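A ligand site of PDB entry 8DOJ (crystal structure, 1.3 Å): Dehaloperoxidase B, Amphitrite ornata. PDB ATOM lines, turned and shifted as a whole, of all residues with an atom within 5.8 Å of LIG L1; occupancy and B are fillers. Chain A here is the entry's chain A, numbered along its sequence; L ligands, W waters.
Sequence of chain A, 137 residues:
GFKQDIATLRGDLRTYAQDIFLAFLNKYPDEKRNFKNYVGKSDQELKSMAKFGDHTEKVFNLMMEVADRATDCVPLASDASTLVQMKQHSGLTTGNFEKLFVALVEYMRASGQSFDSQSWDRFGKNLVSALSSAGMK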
ATOM      1  N   PHE A  24       8.641  -5.083  15.643  1.00  0.00           N
ATOM      2  CA  PHE A  24       9.730  -5.802  14.984  1.00  0.00           C
ATOM      3  C   PHE A  24      10.748  -4.858  14.341  1.00  0.00           C
ATOM      4  O   PHE A  24      11.931  -4.942  14.600  1.00  0.00           O
ATOM      5  CB  PHE A  24       9.124  -6.809  14.000  1.00  0.00           C
ATOM      6  CG  PHE A  24      10.088  -7.394  13.009  1.00  0.00           C
ATOM      7  CD1 PHE A  24      10.999  -8.359  13.402  1.00  0.00           C
ATOM      8  CD2 PHE A  24      10.128  -6.942  11.699  1.00  0.00           C
ATOM      9  CE1 PHE A  24      11.875  -8.923  12.476  1.00  0.00           C
ATOM     10  CE2 PHE A  24      11.003  -7.511  10.782  1.00  0.00           C
ATOM     11  CZ  PHE A  24      11.851  -8.514  11.164  1.00  0.00           C
ATOM     12  N   GLU A  31      16.634  -5.068  10.113  1.00  0.00           N
ATOM     13  CA  GLU A  31      15.679  -5.863   9.371  1.00  0.00           C
ATOM     14  C   GLU A  31      15.063  -5.033   8.222  1.00  0.00           C
ATOM     15  O   GLU A  31      14.478  -5.596   7.309  1.00  0.00           O
ATOM     16  CB  GLU A  31      14.614  -6.487  10.282  1.00  0.00           C
ATOM     17  CG  GLU A  31      15.176  -7.603  11.187  1.00  0.00           C
ATOM     18  CD  GLU A  31      15.684  -8.826  10.433  1.00  0.00           C
ATOM     19  OE1 GLU A  31      16.824  -9.266  10.691  1.00  0.00           O
ATOM     20  OE2 GLU A  31      14.911  -9.338   9.595  1.00  0.00           O
ATOM     21  N   ASN A  34      15.316  -5.600   4.244  1.00  0.00           N
ATOM     22  CA  ASN A  34      14.340  -6.367   3.455  1.00  0.00           C
ATOM     23  C   ASN A  34      13.132  -5.514   3.082  1.00  0.00           C
ATOM     24  O   ASN A  34      12.226  -6.007   2.416  1.00  0.00           O
ATOM     25  CB  ASN A  34      13.778  -7.582   4.217  1.00  0.00           C
ATOM     26  CG  ASN A  34      14.828  -8.395   4.945  1.00  0.00           C
ATOM     27  OD1 ASN A  34      15.569  -9.093   4.256  1.00  0.00           O
ATOM     28  ND2 ASN A  34      14.950  -8.282   6.271  1.00  0.00           N
ATOM     29  N   PHE A  35      13.082  -4.275   3.617  1.00  0.00           N
ATOM     30  CA  PHE A  35      11.924  -3.392   3.492  1.00  0.00           C
ATOM     31  C   PHE A  35      12.388  -1.962   3.220  1.00  0.00           C
ATOM     32  O   PHE A  35      12.058  -1.032   3.958  1.00  0.00           O
ATOM     33  CB  PHE A  35      11.082  -3.470   4.770  1.00  0.00           C
ATOM     34  CG  PHE A  35      10.623  -4.864   5.100  1.00  0.00           C
ATOM     35  CD1 PHE A  35       9.539  -5.406   4.442  1.00  0.00           C
ATOM     36  CD2 PHE A  35      11.249  -5.604   6.092  1.00  0.00           C
ATOM     37  CE1 PHE A  35       9.101  -6.676   4.777  1.00  0.00           C
ATOM     38  CE2 PHE A  35      10.805  -6.872   6.403  1.00  0.00           C
ATOM     39  CZ  PHE A  35       9.763  -7.425   5.724  1.00  0.00           C
ATOM     40  N   TYR A  38      10.459   1.315   3.605  1.00  0.00           N
ATOM     41  CA  TYR A  38      10.034   1.714   4.967  1.00  0.00           C
ATOM     42  C   TYR A  38      11.099   2.530   5.730  1.00  0.00           C
ATOM     43  O   TYR A  38      10.832   3.014   6.820  1.00  0.00           O
ATOM     44  CB  TYR A  38       9.489   0.531   5.774  1.00  0.00           C
ATOM     45  CG  TYR A  38       8.364  -0.198   5.061  1.00  0.00           C
ATOM     46  CD1 TYR A  38       7.571   0.471   4.136  1.00  0.00           C
ATOM     47  CD2 TYR A  38       8.071  -1.522   5.345  1.00  0.00           C
ATOM     48  CE1 TYR A  38       6.551  -0.173   3.455  1.00  0.00           C
ATOM     49  CE2 TYR A  38       7.068  -2.208   4.656  1.00  0.00           C
ATOM     50  CZ  TYR A  38       6.309  -1.527   3.709  1.00  0.00           C
ATOM     51  OH  TYR A  38       5.302  -2.202   3.060  1.00  0.00           O
ATOM     52  N   ASP A  54      -1.501  -2.770   3.644  1.00  0.00           N
ATOM     53  CA  ASP A  54      -2.007  -3.863   2.828  1.00  0.00           C
ATOM     54  C   ASP A  54      -1.179  -5.124   3.036  1.00  0.00           C
ATOM     55  O   ASP A  54      -1.740  -6.182   3.304  1.00  0.00           O
ATOM     56  CB  ASP A  54      -1.975  -3.581   1.314  1.00  0.00           C
ATOM     57  CG  ASP A  54      -2.650  -4.673   0.479  1.00  0.00           C
ATOM     58  OD1 ASP A  54      -3.849  -4.858   0.669  1.00  0.00           O
ATOM     59  OD2 ASP A  54      -1.974  -5.323  -0.372  1.00  0.00           O
ATOM     60  N   HIS A  55       0.121  -5.015   2.797  1.00  0.00           N
ATOM     61  CA  HIS A  55       1.017  -6.153   2.808  1.00  0.00           C
ATOM     62  C   HIS A  55       1.087  -6.688   4.220  1.00  0.00           C
ATOM     63  O   HIS A  55       1.088  -7.902   4.426  1.00  0.00           O
ATOM     64  CB  HIS A  55       2.407  -5.810   2.300  1.00  0.00           C
ATOM     65  CG  HIS A  55       2.454  -5.510   0.834  1.00  0.00           C
ATOM     66  ND1 HIS A  55       3.609  -5.689   0.135  1.00  0.00           N
ATOM     67  CD2 HIS A  55       1.525  -5.096  -0.087  1.00  0.00           C
ATOM     68  CE1 HIS A  55       3.405  -5.446  -1.166  1.00  0.00           C
ATOM     69  NE2 HIS A  55       2.124  -5.081  -1.330  1.00  0.00           N
ATOM     70  N   LYS A  58      -1.862  -8.762   5.028  1.00  0.00           N
ATOM     71  CA  LYS A  58      -1.884 -10.025   4.336  1.00  0.00           C
ATOM     72  C   LYS A  58      -0.872 -11.016   4.932  1.00  0.00           C
ATOM     73  O   LYS A  58      -1.172 -12.204   5.060  1.00  0.00           O
ATOM     74  CB  LYS A  58      -1.607  -9.806   2.845  1.00  0.00           C
ATOM     75  CG  LYS A  58      -2.761  -9.262   2.025  1.00  0.00           C
ATOM     76  CD  LYS A  58      -2.408  -8.999   0.596  1.00  0.00           C
ATOM     77  CE  LYS A  58      -3.551  -8.378  -0.178  1.00  0.00           C
ATOM     78  NZ  LYS A  58      -3.101  -7.866  -1.481  1.00  0.00           N
ATOM     79  N   VAL A  59       0.261 -10.530   5.426  1.00  0.00           N
ATOM     80  CA  VAL A  59       1.195 -11.358   6.182  1.00  0.00           C
ATOM     81  C   VAL A  59       0.505 -11.965   7.396  1.00  0.00           C
ATOM     82  O   VAL A  59       0.597 -13.174   7.610  1.00  0.00           O
ATOM     83  CB  VAL A  59       2.431 -10.513   6.610  1.00  0.00           C
ATOM     84  CG1 VAL A  59       3.295 -11.252   7.636  1.00  0.00           C
ATOM     85  CG2 VAL A  59       3.257 -10.061   5.403  1.00  0.00           C
ATOM     86  N   PHE A  60      -0.194 -11.133   8.171  1.00  0.00           N
ATOM     87  CA  PHE A  60      -0.832 -11.649   9.366  1.00  0.00           C
ATOM     88  C   PHE A  60      -2.081 -12.434   9.075  1.00  0.00           C
ATOM     89  O   PHE A  60      -2.354 -13.389   9.820  1.00  0.00           O
ATOM     90  CB  PHE A  60      -1.124 -10.499  10.342  1.00  0.00           C
ATOM     91  CG  PHE A  60       0.072 -10.156  11.163  1.00  0.00           C
ATOM     92  CD1 PHE A  60       1.148  -9.490  10.640  1.00  0.00           C
ATOM     93  CD2 PHE A  60       0.116 -10.532  12.498  1.00  0.00           C
ATOM     94  CE1 PHE A  60       2.266  -9.213  11.397  1.00  0.00           C
ATOM     95  CE2 PHE A  60       1.233 -10.272  13.245  1.00  0.00           C
ATOM     96  CZ  PHE A  60       2.311  -9.618  12.704  1.00  0.00           C
ATOM     97  N   LEU A  62      -2.242 -14.649   6.691  1.00  0.00           N
ATOM     98  CA  LEU A  62      -1.700 -15.986   6.497  1.00  0.00           C
ATOM     99  C   LEU A  62      -1.115 -16.503   7.784  1.00  0.00           C
ATOM    100  O   LEU A  62      -1.247 -17.703   8.089  1.00  0.00           O
ATOM    101  CB  LEU A  62      -0.660 -15.962   5.366  1.00  0.00           C
ATOM    102  CG  LEU A  62      -0.030 -17.316   5.039  1.00  0.00           C
ATOM    103  CD1 LEU A  62      -1.087 -18.380   4.707  1.00  0.00           C
ATOM    104  CD2 LEU A  62       0.969 -17.202   3.894  1.00  0.00           C
ATOM    105  N   MET A  63      -0.413 -15.679   8.541  1.00  0.00           N
ATOM    106  CA  MET A  63       0.148 -16.161   9.809  1.00  0.00           C
ATOM    107  C   MET A  63      -0.944 -16.773  10.699  1.00  0.00           C
ATOM    108  O   MET A  63      -0.724 -17.817  11.346  1.00  0.00           O
ATOM    109  CB  MET A  63       0.849 -15.031  10.555  1.00  0.00           C
ATOM    110  CG  MET A  63       1.609 -15.513  11.779  1.00  0.00           C
ATOM    111  SD  MET A  63       2.098 -14.210  12.932  1.00  0.00           S
ATOM    112  CE  MET A  63       3.101 -13.158  11.881  1.00  0.00           C
ATOM    113  N   VAL A  66      -1.875 -20.190   9.500  1.00  0.00           N
ATOM    114  CA  VAL A  66      -0.848 -21.175   9.846  1.00  0.00           C
ATOM    115  C   VAL A  66      -0.985 -21.548  11.322  1.00  0.00           C
ATOM    116  O   VAL A  66      -0.905 -22.722  11.717  1.00  0.00           O
ATOM    117  CB  VAL A  66       0.565 -20.651   9.504  1.00  0.00           C
ATOM    118  CG1 VAL A  66       1.651 -21.599   9.963  1.00  0.00           C
ATOM    119  CG2 VAL A  66       0.688 -20.390   7.983  1.00  0.00           C
ATOM    120  N   LEU A  83       5.895 -21.244   3.024  1.00  0.00           N
ATOM    121  CA  LEU A  83       6.650 -20.089   3.467  1.00  0.00           C
ATOM    122  C   LEU A  83       8.102 -20.114   2.995  1.00  0.00           C
ATOM    123  O   LEU A  83       8.646 -19.062   2.696  1.00  0.00           O
ATOM    124  CB  LEU A  83       6.571 -20.003   4.984  1.00  0.00           C
ATOM    125  CG  LEU A  83       5.190 -19.699   5.572  1.00  0.00           C
ATOM    126  CD1 LEU A  83       5.210 -19.837   7.096  1.00  0.00           C
ATOM    127  CD2 LEU A  83       4.657 -18.349   5.121  1.00  0.00           C
ATOM    128  N   MET A  86       7.862 -19.464  -1.222  1.00  0.00           N
ATOM    129  CA  MET A  86       7.349 -18.177  -1.705  1.00  0.00           C
ATOM    130  C   MET A  86       8.479 -17.332  -2.278  1.00  0.00           C
ATOM    131  O   MET A  86       9.456 -17.134  -1.582  1.00  0.00           O
ATOM    132  CB  MET A  86       6.734 -17.385  -0.540  1.00  0.00           C
ATOM    133  CG  MET A  86       5.339 -17.746  -0.219  1.00  0.00           C
ATOM    134  SD  MET A  86       4.875 -16.946   1.329  1.00  0.00           S
ATOM    135  CE  MET A  86       4.864 -15.213   0.883  1.00  0.00           C
ATOM    136  N   GLN A  88       8.716 -14.209  -2.560  1.00  0.00           N
ATOM    137  CA  GLN A  88       8.970 -13.021  -1.762  1.00  0.00           C
ATOM    138  C   GLN A  88       9.870 -13.347  -0.574  1.00  0.00           C
ATOM    139  O   GLN A  88      10.429 -12.425   0.037  1.00  0.00           O
ATOM    140  CB  GLN A  88       7.645 -12.365  -1.348  1.00  0.00           C
ATOM    141  CG  GLN A  88       6.947 -11.658  -2.502  1.00  0.00           C
ATOM    142  CD  GLN A  88       5.466 -11.462  -2.287  1.00  0.00           C
ATOM    143  OE1 GLN A  88       4.743 -12.412  -2.022  1.00  0.00           O
ATOM    144  NE2 GLN A  88       5.002 -10.222  -2.426  1.00  0.00           N
ATOM    145  N   HIS A  89      10.075 -14.637  -0.280  1.00  0.00           N
ATOM    146  CA  HIS A  89      10.925 -15.062   0.842  1.00  0.00           C
ATOM    147  C   HIS A  89      12.283 -15.612   0.401  1.00  0.00           C
ATOM    148  O   HIS A  89      13.008 -16.214   1.211  1.00  0.00           O
ATOM    149  CB  HIS A  89      10.185 -16.118   1.673  1.00  0.00           C
ATOM    150  CG  HIS A  89       9.045 -15.559   2.452  1.00  0.00           C
ATOM    151  ND1 HIS A  89       8.166 -16.335   3.160  1.00  0.00           N
ATOM    152  CD2 HIS A  89       8.630 -14.265   2.658  1.00  0.00           C
ATOM    153  CE1 HIS A  89       7.253 -15.567   3.752  1.00  0.00           C
ATOM    154  NE2 HIS A  89       7.588 -14.272   3.518  1.00  0.00           N
ATOM    155  N   LEU A  92      15.564 -15.030   2.505  1.00  0.00           N
ATOM    156  CA  LEU A  92      15.388 -14.994   3.952  1.00  0.00           C
ATOM    157  C   LEU A  92      16.067 -16.186   4.625  1.00  0.00           C
ATOM    158  O   LEU A  92      16.313 -17.202   3.998  1.00  0.00           O
ATOM    159  CB  LEU A  92      13.891 -14.972   4.309  1.00  0.00           C
ATOM    160  CG  LEU A  92      13.096 -13.765   3.832  1.00  0.00           C
ATOM    161  CD1 LEU A  92      11.695 -13.792   4.413  1.00  0.00           C
ATOM    162  CD2 LEU A  92      13.762 -12.451   4.220  1.00  0.00           C
ATOM    163  N   ASN A  96      15.408 -14.320  10.507  1.00  0.00           N
ATOM    164  CA  ASN A  96      14.413 -13.286  10.255  1.00  0.00           C
ATOM    165  C   ASN A  96      13.093 -13.596  10.946  1.00  0.00           C
ATOM    166  O   ASN A  96      12.429 -12.699  11.508  1.00  0.00           O
ATOM    167  CB  ASN A  96      14.156 -13.165   8.745  1.00  0.00           C
ATOM    168  CG  ASN A  96      15.364 -12.699   7.946  1.00  0.00           C
ATOM    169  OD1 ASN A  96      15.914 -13.440   7.136  1.00  0.00           O
ATOM    170  ND2 ASN A  96      15.759 -11.448   8.129  1.00  0.00           N
ATOM    171  N   PHE A  97      12.672 -14.886  10.852  1.00  0.00           N
ATOM    172  CA  PHE A  97      11.455 -15.338  11.506  1.00  0.00           C
ATOM    173  C   PHE A  97      11.575 -15.385  13.031  1.00  0.00           C
ATOM    174  O   PHE A  97      10.643 -15.017  13.717  1.00  0.00           O
ATOM    175  CB  PHE A  97      11.015 -16.685  10.931  1.00  0.00           C
ATOM    176  CG  PHE A  97      10.559 -16.629   9.498  1.00  0.00           C
ATOM    177  CD1 PHE A  97      11.508 -16.541   8.480  1.00  0.00           C
ATOM    178  CD2 PHE A  97       9.216 -16.634   9.157  1.00  0.00           C
ATOM    179  CE1 PHE A  97      11.105 -16.402   7.163  1.00  0.00           C
ATOM    180  CE2 PHE A  97       8.819 -16.549   7.833  1.00  0.00           C
ATOM    181  CZ  PHE A  97       9.767 -16.449   6.834  1.00  0.00           C
ATOM    182  N   LEU A 100      10.970 -11.916  14.234  1.00  0.00           N
ATOM    183  CA  LEU A 100       9.568 -11.528  14.153  1.00  0.00           C
ATOM    184  C   LEU A 100       8.861 -12.016  15.421  1.00  0.00           C
ATOM    185  O   LEU A 100       8.151 -11.248  16.087  1.00  0.00           O
ATOM    186  CB  LEU A 100       8.964 -12.093  12.862  1.00  0.00           C
ATOM    187  CG  LEU A 100       7.447 -12.038  12.721  1.00  0.00           C
ATOM    188  CD1 LEU A 100       7.012 -12.376  11.312  1.00  0.00           C
ATOM    189  CD2 LEU A 100       6.732 -12.995  13.660  1.00  0.00           C
ATOM    190  N   PHE A 101       9.076 -13.312  15.783  1.00  0.00           N
ATOM    191  CA  PHE A 101       8.377 -13.927  16.910  1.00  0.00           C
ATOM    192  C   PHE A 101       8.868 -13.405  18.259  1.00  0.00           C
ATOM    193  O   PHE A 101       8.036 -13.275  19.156  1.00  0.00           O
ATOM    194  CB  PHE A 101       8.294 -15.454  16.779  1.00  0.00           C
ATOM    195  CG  PHE A 101       7.263 -15.847  15.762  1.00  0.00           C
ATOM    196  CD1 PHE A 101       5.910 -15.853  16.084  1.00  0.00           C
ATOM    197  CD2 PHE A 101       7.621 -16.028  14.442  1.00  0.00           C
ATOM    198  CE1 PHE A 101       4.955 -16.043  15.092  1.00  0.00           C
ATOM    199  CE2 PHE A 101       6.660 -16.250  13.466  1.00  0.00           C
ATOM    200  CZ  PHE A 101       5.327 -16.258  13.791  1.00  0.00           C
ATOM    201  N   PHE A 123       5.106 -21.501  19.368  1.00  0.00           N
ATOM    202  CA  PHE A 123       4.759 -21.463  17.945  1.00  0.00           C
ATOM    203  C   PHE A 123       5.927 -20.928  17.108  1.00  0.00           C
ATOM    204  O   PHE A 123       6.289 -21.454  16.047  1.00  0.00           O
ATOM    205  CB  PHE A 123       3.484 -20.654  17.732  1.00  0.00           C
ATOM    206  CG  PHE A 123       3.086 -20.526  16.293  1.00  0.00           C
ATOM    207  CD1 PHE A 123       2.675 -21.626  15.527  1.00  0.00           C
ATOM    208  CD2 PHE A 123       3.012 -19.268  15.691  1.00  0.00           C
ATOM    209  CE1 PHE A 123       2.329 -21.475  14.169  1.00  0.00           C
ATOM    210  CE2 PHE A 123       2.653 -19.126  14.349  1.00  0.00           C
ATOM    211  CZ  PHE A 123       2.258 -20.212  13.617  1.00  0.00           C
ATOM    212  N   LEU A 127       7.763 -23.032  14.363  1.00  0.00           N
ATOM    213  CA  LEU A 127       7.722 -22.599  12.968  1.00  0.00           C
ATOM    214  C   LEU A 127       9.155 -22.483  12.432  1.00  0.00           C
ATOM    215  O   LEU A 127       9.469 -22.991  11.361  1.00  0.00           O
ATOM    216  CB  LEU A 127       6.981 -21.287  12.830  1.00  0.00           C
ATOM    217  CG  LEU A 127       6.962 -20.760  11.411  1.00  0.00           C
ATOM    218  CD1 LEU A 127       6.266 -21.711  10.454  1.00  0.00           C
ATOM    219  CD2 LEU A 127       6.268 -19.406  11.399  1.00  0.00           C
HETATM  220  C1  LIG L   1       5.669 -10.953   1.581  1.00  0.00           C
HETATM  221  C2  LIG L   1       3.570 -14.064   4.714  1.00  0.00           C
HETATM  222  C3  LIG L   1       7.379 -13.629   7.664  1.00  0.00           C
HETATM  223  C4  LIG L   1       9.662 -10.805   4.402  1.00  0.00           C
HETATM  224  C5  LIG L   1       4.741 -11.763   2.249  1.00  0.00           C
HETATM  225  C6  LIG L   1       3.383 -11.976   1.809  1.00  0.00           C
HETATM  226  C7  LIG L   1       2.798 -12.854   2.667  1.00  0.00           C
HETATM  227  C8  LIG L   1       3.790 -13.182   3.637  1.00  0.00           C
HETATM  228  C9  LIG L   1       1.396 -13.351   2.581  1.00  0.00           C
HETATM  229  C10 LIG L   1       2.767 -11.263   0.581  1.00  0.00           C
HETATM  230  C11 LIG L   1       2.303  -9.865   0.989  1.00  0.00           C
HETATM  231  C12 LIG L   1       1.744  -9.106  -0.179  1.00  0.00           C
HETATM  232  O1  LIG L   1       0.797  -8.332   0.002  1.00  0.00           O
HETATM  233  O2  LIG L   1       2.210  -9.163  -1.314  1.00  0.00           O
HETATM  234  C13 LIG L   1       4.453 -14.231   5.768  1.00  0.00           C
HETATM  235  C14 LIG L   1       4.123 -14.995   6.985  1.00  0.00           C
HETATM  236  C15 LIG L   1       5.175 -14.858   7.825  1.00  0.00           C
HETATM  237  C16 LIG L   1       6.172 -14.033   7.109  1.00  0.00           C
HETATM  238  C17 LIG L   1       2.849 -15.734   7.276  1.00  0.00           C
HETATM  239  C18 LIG L   1       5.391 -15.425   9.188  1.00  0.00           C
HETATM  240  C19 LIG L   1       4.836 -16.511   9.687  1.00  0.00           C
HETATM  241  C20 LIG L   1       8.274 -12.801   7.024  1.00  0.00           C
HETATM  242  C21 LIG L   1       9.487 -12.379   7.626  1.00  0.00           C
HETATM  243  C22 LIG L   1      10.135 -11.596   6.691  1.00  0.00           C
HETATM  244  C23 LIG L   1       9.269 -11.492   5.546  1.00  0.00           C
HETATM  245  C24 LIG L   1      10.046 -12.775   8.965  1.00  0.00           C
HETATM  246  C25 LIG L   1      11.401 -10.852   6.832  1.00  0.00           C
HETATM  247  C26 LIG L   1      11.894 -10.442   8.014  1.00  0.00           C
HETATM  248  C27 LIG L   1       8.724 -10.700   3.337  1.00  0.00           C
HETATM  249  C28 LIG L   1       8.997  -9.783   2.197  1.00  0.00           C
HETATM  250  C29 LIG L   1       7.892  -9.818   1.440  1.00  0.00           C
HETATM  251  C30 LIG L   1       6.927 -10.697   2.108  1.00  0.00           C
HETATM  252  C31 LIG L   1      10.236  -8.979   1.913  1.00  0.00           C
HETATM  253  C32 LIG L   1       7.623  -9.045   0.161  1.00  0.00           C
HETATM  254  C33 LIG L   1       7.868  -7.544   0.273  1.00  0.00           C
HETATM  255  C34 LIG L   1       6.657  -6.892   0.893  1.00  0.00           C
HETATM  256  O3  LIG L   1       5.592  -7.562   0.960  1.00  0.00           O
HETATM  257  O4  LIG L   1       6.718  -5.723   1.305  1.00  0.00           O
HETATM  258  N1  LIG L   1       4.963 -12.539   3.353  1.00  0.00           N
HETATM  259  N2  LIG L   1       5.661 -13.689   5.900  1.00  0.00           N
HETATM  260  N3  LIG L   1       8.145 -12.239   5.768  1.00  0.00           N
HETATM  261  N4  LIG L   1       7.449 -11.235   3.255  1.00  0.00           N
HETATM  262 FE1  LIG L   1       6.661 -12.611   4.442  1.00  0.00          FE
HETATM  263  O1  LG2 L   2       4.553  -5.795   5.416  1.00  0.00           O
HETATM  264  C1  LG2 L   2       5.605  -7.304   6.914  1.00  0.00           C
HETATM  265  O2  LG2 L   2       5.502  -8.670  11.964  1.00  0.00           O
HETATM  266  C2  LG2 L   2       5.260  -6.946   5.617  1.00  0.00           C
HETATM  267  C3  LG2 L   2       6.440  -8.865   4.814  1.00  0.00           C
HETATM  268  C4  LG2 L   2       6.388  -8.842  10.937  1.00  0.00           C
HETATM  269  C5  LG2 L   2       5.938  -8.624   9.645  1.00  0.00           C
HETATM  270  C6  LG2 L   2       8.570  -9.301  10.099  1.00  0.00           C
HETATM  271  C7  LG2 L   2       6.806  -8.758   8.554  1.00  0.00           C
HETATM  272  C8  LG2 L   2       6.354  -8.459   7.180  1.00  0.00           C
HETATM  273  C9  LG2 L   2       6.760  -9.271   6.115  1.00  0.00           C
HETATM  274  C10 LG2 L   2       5.643  -7.775   4.562  1.00  0.00           C
HETATM  275  C11 LG2 L   2       8.117  -9.113   8.800  1.00  0.00           C
HETATM  276  C12 LG2 L   2       7.715  -9.140  11.184  1.00  0.00           C
HETATM  277  O   HOH W   1       6.018  -3.861  -1.115  1.00  0.00           O
HETATM  278  O   HOH W   2      -0.401  -7.308  -2.012  1.00  0.00           O
HETATM  279  O   HOH W   3       5.437  -4.639   3.163  1.00  0.00           O
HETATM  280  O   HOH W   4      10.630  -5.583   0.451  1.00  0.00           O
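An oxygen (O3) of LIG L1 sits at hydrogen-bond distance from a ring nitrogen (ND1) of His 55.
A ring nitrogen (NE2) of His 89 is bound to an iron atom (FE1) of LIG L1 (2.1 Å).
The side-chain amide nitrogen (NE2) of Gln 88 lies within hydrogen-bond range of an oxygen (O2) of LIG L1 (3.2 Å).
A ring nitrogen (ND1) of His 89 lies within hydrogen-bond range of the backbone carbonyl oxygen (O) of Leu 83 (2.8 Å).
The side-chain carboxylate (OE2) of Glu 31 lies within hydrogen-bond range of the side-chain amide nitrogen (ND2) of Asn 96, at 2.7 Å.
The side-chain carboxylate (OD2) of Asp 54 is in salt-bridge range of the side-chain amino group (NZ) of Lys 58 (3.0 Å).
The backbone carbonyl oxygen of Glu 31 sits at hydrogen-bond distance from the side-chain amide nitrogen of Asn 34 (2.9 Å).
Phe 24 touches LIG L1.
Glu 31 touches LIG L1 (OE2 to C26, 3.6 Å).
O of Asn 34 touches C31 of LIG L1, 3.6 Å away.
Phe 35 touches LIG L1.
Lys 58 touches LIG L1.
Val 59 touches LIG L1.
Leu 62 touches LIG L1 (CG to C17, 3.97 Å).
Met 63 touches LIG L1.
CD2 of Leu 83 touches C17 of LIG L1, at 3.8 Å.
Met 86 touches LIG L1 (CE to C8, 3.6 Å).
CD1 of Leu 92 touches C22 of LIG L1, 3.5 Å away.
Asn 96 touches LIG L1 (O to C24, 3.5 Å).
CE2 of Phe 97 touches C3 of LIG L1, at 3.3 Å.
Leu 100 touches LIG L1.
Leu 127 touches LIG L1 (CD2 to C19, 3.7 Å).
Hydrophobic or aromatic side chains that line LIG L1: Phe 24, Phe 35, His 55, Val 59, Leu 62, Met 63, Leu 83, Met 86, His 89, Leu 92, Phe 97, Leu 100 and Leu 127.
18 residues have an atom within 4 Å of LIG L1: Phe 24, Glu 31, Asn 34, Phe 35, His 55, Lys 58, Val 59, Leu 62, Met 63, Leu 83, Met 86, Gln 88, His 89, Leu 92, Asn 96, Phe 97, Leu 100 and Leu 127.
Water W3 lies within hydrogen-bond range of the side-chain hydroxyl of Tyr 38 (2.4 Å), an oxygen (O4) of LIG L1 (2.5 Å) and an oxygen (O1) of LG2 L2 (2.7 Å).
Water W2 lies within hydrogen-bond range of an oxygen (O1) of LIG L1 (2.6 Å), the side-chain amino group of Lys 58 (2.8 Å), the side-chain carboxylate of Asp 54 (3.0 Å) and a ring nitrogen (NE2) of His 55 (3.4 Å).
Water W1 lies within hydrogen-bond range of an oxygen (O4) of LIG L1 (3.1 Å) and a ring nitrogen (ND1) of His 55 (3.3 Å).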
